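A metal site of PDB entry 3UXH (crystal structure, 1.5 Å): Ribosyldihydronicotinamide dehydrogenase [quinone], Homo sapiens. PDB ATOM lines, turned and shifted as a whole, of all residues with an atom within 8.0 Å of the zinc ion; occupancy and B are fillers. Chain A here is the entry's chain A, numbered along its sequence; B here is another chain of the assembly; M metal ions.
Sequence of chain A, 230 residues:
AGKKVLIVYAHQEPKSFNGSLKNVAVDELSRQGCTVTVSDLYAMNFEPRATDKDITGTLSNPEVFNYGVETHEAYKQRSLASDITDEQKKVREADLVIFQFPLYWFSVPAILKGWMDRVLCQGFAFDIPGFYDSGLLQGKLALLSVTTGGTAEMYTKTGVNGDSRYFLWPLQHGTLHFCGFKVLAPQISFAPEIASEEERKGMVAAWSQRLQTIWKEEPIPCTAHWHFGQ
NE2 of His 177 sits at hydrogen-bond distance from OD1 of Asp 133. The backbone carbonyl oxygen (O) of Thr 223 is in hydrogen-bond range of a ring nitrogen (ND1) of His 227 (2.9 Å). The backbone carbonyl oxygen (O) of His 173 lies within hydrogen-bond range of the backbone NH (N) of Phe 178. A ring nitrogen (NE2) of His 173 sits at hydrogen-bond distance from the backbone carbonyl oxygen (O) of Val 160 of chain B (3.0 Å). SG of Cys 222 sits close to O of Gln 172. OG1 of Thr 223 is in hydrogen-bond range of O of Pro 221. The side-chain hydroxyl of Thr 223 sits at hydrogen-bond distance from the backbone NH of Trp 226 (3.0 Å). N of His 177 lies within hydrogen-bond range of O of Gln 172 (2.7 Å).
Merely in contact with the zinc ion: Thr 223. Four residues have an atom within 4 Å of the zinc ion: His 173, His 177, Cys 222 and Thr 223. Along chain A the residues within 4 Å of the zinc ion span positions 173 to 223.
O of Cys 222 binds the zinc ion, at 2.0 Å. The zinc ion is bound by ND1 of His 173. The zinc ion is bound by ND1 of His 177, 2.2 Å away. The side-chain sulfur (SG) of Cys 222 binds the zinc ion. The zinc ion has four donor atoms within binding distance.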
ATOM      1  N   TYR A 132     -19.296   5.137  12.073  1.00  0.00           N
ATOM      2  CA  TYR A 132     -20.187   6.209  12.580  1.00  0.00           C
ATOM      3  C   TYR A 132     -21.410   6.286  11.707  1.00  0.00           C
ATOM      4  O   TYR A 132     -22.165   5.273  11.628  1.00  0.00           O
ATOM      5  CB  TYR A 132     -19.454   7.635  12.757  1.00  0.00           C
ATOM      6  CG  TYR A 132     -18.465   7.623  13.877  1.00  0.00           C
ATOM      7  CD1 TYR A 132     -18.879   7.364  15.164  1.00  0.00           C
ATOM      8  CD2 TYR A 132     -17.113   7.809  13.633  1.00  0.00           C
ATOM      9  CE1 TYR A 132     -17.945   7.288  16.229  1.00  0.00           C
ATOM     10  CE2 TYR A 132     -16.155   7.728  14.684  1.00  0.00           C
ATOM     11  CZ  TYR A 132     -16.610   7.506  15.957  1.00  0.00           C
ATOM     12  OH  TYR A 132     -15.703   7.444  16.999  1.00  0.00           O
ATOM     13  N   ASP A 133     -21.696   7.421  11.062  1.00  0.00           N
ATOM     14  CA  ASP A 133     -22.999   7.441  10.345  1.00  0.00           C
ATOM     15  C   ASP A 133     -22.980   6.516   9.124  1.00  0.00           C
ATOM     16  O   ASP A 133     -24.030   6.249   8.528  1.00  0.00           O
ATOM     17  CB  ASP A 133     -23.330   8.863   9.941  1.00  0.00           C
ATOM     18  CG  ASP A 133     -23.617   9.755  11.130  1.00  0.00           C
ATOM     19  OD1 ASP A 133     -23.793   9.234  12.270  1.00  0.00           O
ATOM     20  OD2 ASP A 133     -23.668  10.988  10.879  1.00  0.00           O
ATOM     21  N   TRP A 169     -18.912   8.009  27.164  1.00  0.00           N
ATOM     22  CA  TRP A 169     -18.341   8.290  25.852  1.00  0.00           C
ATOM     23  C   TRP A 169     -17.860   7.040  25.126  1.00  0.00           C
ATOM     24  O   TRP A 169     -18.221   6.843  23.978  1.00  0.00           O
ATOM     25  CB  TRP A 169     -17.260   9.399  25.963  1.00  0.00           C
ATOM     26  CG  TRP A 169     -16.489   9.740  24.700  1.00  0.00           C
ATOM     27  CD1 TRP A 169     -15.155   9.416  24.440  1.00  0.00           C
ATOM     28  CD2 TRP A 169     -16.922  10.503  23.590  1.00  0.00           C
ATOM     29  NE1 TRP A 169     -14.750   9.980  23.275  1.00  0.00           N
ATOM     30  CE2 TRP A 169     -15.813  10.630  22.692  1.00  0.00           C
ATOM     31  CE3 TRP A 169     -18.153  11.082  23.236  1.00  0.00           C
ATOM     32  CZ2 TRP A 169     -15.873  11.342  21.485  1.00  0.00           C
ATOM     33  CZ3 TRP A 169     -18.213  11.803  22.025  1.00  0.00           C
ATOM     34  CH2 TRP A 169     -17.083  11.928  21.177  1.00  0.00           C
ATOM     35  N   LEU A 171     -18.624   3.987  25.344  1.00  0.00           N
ATOM     36  CA  LEU A 171     -19.674   3.000  25.050  1.00  0.00           C
ATOM     37  C   LEU A 171     -20.668   3.626  24.020  1.00  0.00           C
ATOM     38  O   LEU A 171     -20.935   3.040  23.004  1.00  0.00           O
ATOM     39  CB  LEU A 171     -20.409   2.656  26.335  1.00  0.00           C
ATOM     40  CG  LEU A 171     -19.452   2.061  27.388  1.00  0.00           C
ATOM     41  CD1 LEU A 171     -20.193   1.990  28.741  1.00  0.00           C
ATOM     42  CD2 LEU A 171     -19.134   0.644  26.950  1.00  0.00           C
ATOM     43  N   GLN A 172     -21.159   4.818  24.293  1.00  0.00           N
ATOM     44  CA  GLN A 172     -22.174   5.416  23.412  1.00  0.00           C
ATOM     45  C   GLN A 172     -21.554   5.878  22.097  1.00  0.00           C
ATOM     46  O   GLN A 172     -22.123   5.548  20.961  1.00  0.00           O
ATOM     47  CB  GLN A 172     -22.876   6.605  24.140  1.00  0.00           C
ATOM     48  CG  GLN A 172     -23.788   6.096  25.302  1.00  0.00           C
ATOM     49  CD  GLN A 172     -24.682   7.106  25.844  1.00  0.00           C
ATOM     50  OE1 GLN A 172     -24.386   8.370  25.733  1.00  0.00           O
ATOM     51  NE2 GLN A 172     -25.735   6.643  26.512  1.00  0.00           N
ATOM     52  N   HIS A 173     -20.447   6.637  22.163  1.00  0.00           N
ATOM     53  CA  HIS A 173     -19.841   7.134  20.941  1.00  0.00           C
ATOM     54  C   HIS A 173     -18.885   6.129  20.303  1.00  0.00           C
ATOM     55  O   HIS A 173     -19.035   5.788  19.088  1.00  0.00           O
ATOM     56  CB  HIS A 173     -19.132   8.422  21.232  1.00  0.00           C
ATOM     57  CG  HIS A 173     -18.615   9.112  19.978  1.00  0.00           C
ATOM     58  ND1 HIS A 173     -19.453   9.743  19.073  1.00  0.00           N
ATOM     59  CD2 HIS A 173     -17.385   9.176  19.443  1.00  0.00           C
ATOM     60  CE1 HIS A 173     -18.738  10.238  18.066  1.00  0.00           C
ATOM     61  NE2 HIS A 173     -17.466   9.923  18.273  1.00  0.00           N
ATOM     62  N   GLY A 174     -17.869   5.746  21.101  1.00  0.00           N
ATOM     63  CA  GLY A 174     -16.814   4.907  20.422  1.00  0.00           C
ATOM     64  C   GLY A 174     -17.279   3.556  19.974  1.00  0.00           C
ATOM     65  O   GLY A 174     -16.624   2.942  19.120  1.00  0.00           O
ATOM     66  N   THR A 175     -18.365   3.052  20.618  1.00  0.00           N
ATOM     67  CA  THR A 175     -18.879   1.740  20.242  1.00  0.00           C
ATOM     68  C   THR A 175     -20.196   1.804  19.527  1.00  0.00           C
ATOM     69  O   THR A 175     -20.235   1.482  18.310  1.00  0.00           O
ATOM     70  CB  THR A 175     -19.002   0.876  21.495  1.00  0.00           C
ATOM     71  OG1 THR A 175     -17.726   0.859  22.193  1.00  0.00           O
ATOM     72  CG2 THR A 175     -19.376  -0.554  21.178  1.00  0.00           C
ATOM     73  N   LEU A 176     -21.240   2.284  20.193  1.00  0.00           N
ATOM     74  CA  LEU A 176     -22.616   2.181  19.573  1.00  0.00           C
ATOM     75  C   LEU A 176     -22.720   3.083  18.359  1.00  0.00           C
ATOM     76  O   LEU A 176     -23.119   2.657  17.280  1.00  0.00           O
ATOM     77  CB  LEU A 176     -23.679   2.478  20.626  1.00  0.00           C
ATOM     78  CG  LEU A 176     -23.629   1.443  21.802  1.00  0.00           C
ATOM     79  CD1 LEU A 176     -24.612   1.883  22.863  1.00  0.00           C
ATOM     80  CD2 LEU A 176     -23.994   0.050  21.384  1.00  0.00           C
ATOM     81  N   HIS A 177     -22.372   4.347  18.525  1.00  0.00           N
ATOM     82  CA  HIS A 177     -22.446   5.294  17.344  1.00  0.00           C
ATOM     83  C   HIS A 177     -21.505   4.816  16.211  1.00  0.00           C
ATOM     84  O   HIS A 177     -21.859   4.879  14.986  1.00  0.00           O
ATOM     85  CB  HIS A 177     -22.035   6.680  17.743  1.00  0.00           C
ATOM     86  CG  HIS A 177     -22.265   7.729  16.683  1.00  0.00           C
ATOM     87  ND1 HIS A 177     -21.989   9.043  16.922  1.00  0.00           N
ATOM     88  CD2 HIS A 177     -22.755   7.670  15.417  1.00  0.00           C
ATOM     89  CE1 HIS A 177     -22.265   9.768  15.855  1.00  0.00           C
ATOM     90  NE2 HIS A 177     -22.761   8.963  14.933  1.00  0.00           N
ATOM     91  N   PHE A 178     -20.317   4.350  16.577  1.00  0.00           N
ATOM     92  CA  PHE A 178     -19.333   3.901  15.520  1.00  0.00           C
ATOM     93  C   PHE A 178     -19.923   2.811  14.609  1.00  0.00           C
ATOM     94  O   PHE A 178     -19.659   2.783  13.407  1.00  0.00           O
ATOM     95  CB  PHE A 178     -18.047   3.395  16.201  1.00  0.00           C
ATOM     96  CG  PHE A 178     -16.939   3.021  15.255  1.00  0.00           C
ATOM     97  CD1 PHE A 178     -15.980   3.949  14.900  1.00  0.00           C
ATOM     98  CD2 PHE A 178     -16.795   1.676  14.835  1.00  0.00           C
ATOM     99  CE1 PHE A 178     -14.930   3.622  13.966  1.00  0.00           C
ATOM    100  CE2 PHE A 178     -15.713   1.307  13.958  1.00  0.00           C
ATOM    101  CZ  PHE A 178     -14.792   2.289  13.572  1.00  0.00           C
ATOM    102  N   PHE A 181     -25.442   2.673  15.211  1.00  0.00           N
ATOM    103  CA  PHE A 181     -26.618   2.826  16.083  1.00  0.00           C
ATOM    104  C   PHE A 181     -26.992   4.238  16.398  1.00  0.00           C
ATOM    105  O   PHE A 181     -26.113   5.119  16.526  1.00  0.00           O
ATOM    106  CB  PHE A 181     -26.431   2.197  17.476  1.00  0.00           C
ATOM    107  CG  PHE A 181     -26.408   0.693  17.528  1.00  0.00           C
ATOM    108  CD1 PHE A 181     -27.606  -0.039  17.638  1.00  0.00           C
ATOM    109  CD2 PHE A 181     -25.182   0.001  17.617  1.00  0.00           C
ATOM    110  CE1 PHE A 181     -27.590  -1.442  17.781  1.00  0.00           C
ATOM    111  CE2 PHE A 181     -25.174  -1.407  17.749  1.00  0.00           C
ATOM    112  CZ  PHE A 181     -26.387  -2.120  17.825  1.00  0.00           C
ATOM    113  N   VAL A 183     -28.643   6.173  19.475  1.00  0.00           N
ATOM    114  CA  VAL A 183     -28.480   5.927  20.890  1.00  0.00           C
ATOM    115  C   VAL A 183     -29.576   6.567  21.690  1.00  0.00           C
ATOM    116  O   VAL A 183     -29.682   7.810  21.686  1.00  0.00           O
ATOM    117  CB  VAL A 183     -27.086   6.412  21.388  1.00  0.00           C
ATOM    118  CG1 VAL A 183     -26.980   6.181  22.869  1.00  0.00           C
ATOM    119  CG2 VAL A 183     -25.970   5.574  20.658  1.00  0.00           C
ATOM    120  N   ILE A 220     -30.433  10.526  21.290  1.00  0.00           N
ATOM    121  CA  ILE A 220     -29.539  11.660  21.631  1.00  0.00           C
ATOM    122  C   ILE A 220     -28.693  12.030  20.441  1.00  0.00           C
ATOM    123  O   ILE A 220     -28.461  11.231  19.521  1.00  0.00           O
ATOM    124  CB  ILE A 220     -28.647  11.330  22.840  1.00  0.00           C
ATOM    125  CG1 ILE A 220     -27.590  10.251  22.564  1.00  0.00           C
ATOM    126  CG2 ILE A 220     -29.443  11.032  24.103  1.00  0.00           C
ATOM    127  CD1 ILE A 220     -26.519  10.251  23.634  1.00  0.00           C
ATOM    128  N   PRO A 221     -28.204  13.299  20.431  1.00  0.00           N
ATOM    129  CA  PRO A 221     -27.181  13.676  19.458  1.00  0.00           C
ATOM    130  C   PRO A 221     -25.852  13.131  20.011  1.00  0.00           C
ATOM    131  O   PRO A 221     -25.368  13.669  20.990  1.00  0.00           O
ATOM    132  CB  PRO A 221     -27.224  15.211  19.488  1.00  0.00           C
ATOM    133  CG  PRO A 221     -27.732  15.611  20.924  1.00  0.00           C
ATOM    134  CD  PRO A 221     -28.531  14.349  21.417  1.00  0.00           C
ATOM    135  N   CYS A 222     -25.338  12.032  19.454  1.00  0.00           N
ATOM    136  CA  CYS A 222     -24.216  11.346  20.110  1.00  0.00           C
ATOM    137  C   CYS A 222     -22.910  12.059  19.704  1.00  0.00           C
ATOM    138  O   CYS A 222     -22.128  11.613  18.816  1.00  0.00           O
ATOM    139  CB  CYS A 222     -24.206   9.863  19.743  1.00  0.00           C
ATOM    140  SG  CYS A 222     -22.857   8.917  20.534  1.00  0.00           S
ATOM    141  N   THR A 223     -22.737  13.205  20.336  1.00  0.00           N
ATOM    142  CA  THR A 223     -21.687  14.127  19.994  1.00  0.00           C
ATOM    143  C   THR A 223     -20.781  14.388  21.207  1.00  0.00           C
ATOM    144  O   THR A 223     -21.174  14.199  22.373  1.00  0.00           O
ATOM    145  CB  THR A 223     -22.325  15.514  19.549  1.00  0.00           C
ATOM    146  OG1 THR A 223     -22.997  16.164  20.660  1.00  0.00           O
ATOM    147  CG2 THR A 223     -23.246  15.371  18.363  1.00  0.00           C
ATOM    148  N   ALA A 224     -19.570  14.930  20.966  1.00  0.00           N
ATOM    149  CA  ALA A 224     -18.743  15.375  22.099  1.00  0.00           C
ATOM    150  C   ALA A 224     -19.435  16.454  22.961  1.00  0.00           C
ATOM    151  O   ALA A 224     -19.309  16.479  24.216  1.00  0.00           O
ATOM    152  CB  ALA A 224     -17.320  15.891  21.601  1.00  0.00           C
ATOM    153  N   TRP A 226     -22.668  16.762  23.560  1.00  0.00           N
ATOM    154  CA  TRP A 226     -23.608  16.126  24.478  1.00  0.00           C
ATOM    155  C   TRP A 226     -22.899  15.541  25.719  1.00  0.00           C
ATOM    156  O   TRP A 226     -23.393  15.647  26.866  1.00  0.00           O
ATOM    157  CB  TRP A 226     -24.384  15.011  23.773  1.00  0.00           C
ATOM    158  CG  TRP A 226     -25.501  14.412  24.589  1.00  0.00           C
ATOM    159  CD1 TRP A 226     -26.820  14.829  24.562  1.00  0.00           C
ATOM    160  CD2 TRP A 226     -25.430  13.325  25.548  1.00  0.00           C
ATOM    161  NE1 TRP A 226     -27.557  14.059  25.439  1.00  0.00           N
ATOM    162  CE2 TRP A 226     -26.754  13.120  26.048  1.00  0.00           C
ATOM    163  CE3 TRP A 226     -24.385  12.467  26.009  1.00  0.00           C
ATOM    164  CZ2 TRP A 226     -27.055  12.140  27.027  1.00  0.00           C
ATOM    165  CZ3 TRP A 226     -24.687  11.472  26.949  1.00  0.00           C
ATOM    166  CH2 TRP A 226     -26.024  11.298  27.446  1.00  0.00           C
ATOM    167  N   HIS A 227     -21.751  14.877  25.491  1.00  0.00           N
ATOM    168  CA  HIS A 227     -21.066  14.206  26.594  1.00  0.00           C
ATOM    169  C   HIS A 227     -20.287  15.136  27.537  1.00  0.00           C
ATOM    170  O   HIS A 227     -20.200  14.873  28.741  1.00  0.00           O
ATOM    171  CB  HIS A 227     -20.115  13.112  26.056  1.00  0.00           C
ATOM    172  CG  HIS A 227     -20.849  11.941  25.460  1.00  0.00           C
ATOM    173  ND1 HIS A 227     -21.322  11.928  24.147  1.00  0.00           N
ATOM    174  CD2 HIS A 227     -21.130  10.713  25.968  1.00  0.00           C
ATOM    175  CE1 HIS A 227     -21.919  10.759  23.915  1.00  0.00           C
ATOM    176  NE2 HIS A 227     -21.820  10.011  25.002  1.00  0.00           N
ATOM    177  N   VAL B 160     -13.278  12.749  14.100  1.00  0.00           N
ATOM    178  CA  VAL B 160     -14.437  11.824  14.240  1.00  0.00           C
ATOM    179  C   VAL B 160     -14.463  11.094  15.564  1.00  0.00           C
ATOM    180  O   VAL B 160     -15.554  10.762  16.073  1.00  0.00           O
ATOM    181  CB  VAL B 160     -14.605  10.829  13.055  1.00  0.00           C
ATOM    182  CG1 VAL B 160     -15.032  11.533  11.794  1.00  0.00           C
ATOM    183  CG2 VAL B 160     -13.335   9.999  12.845  1.00  0.00           C
HETATM  184 ZN    ZN M   1     -21.488   9.677  18.925  1.00  0.00          ZN
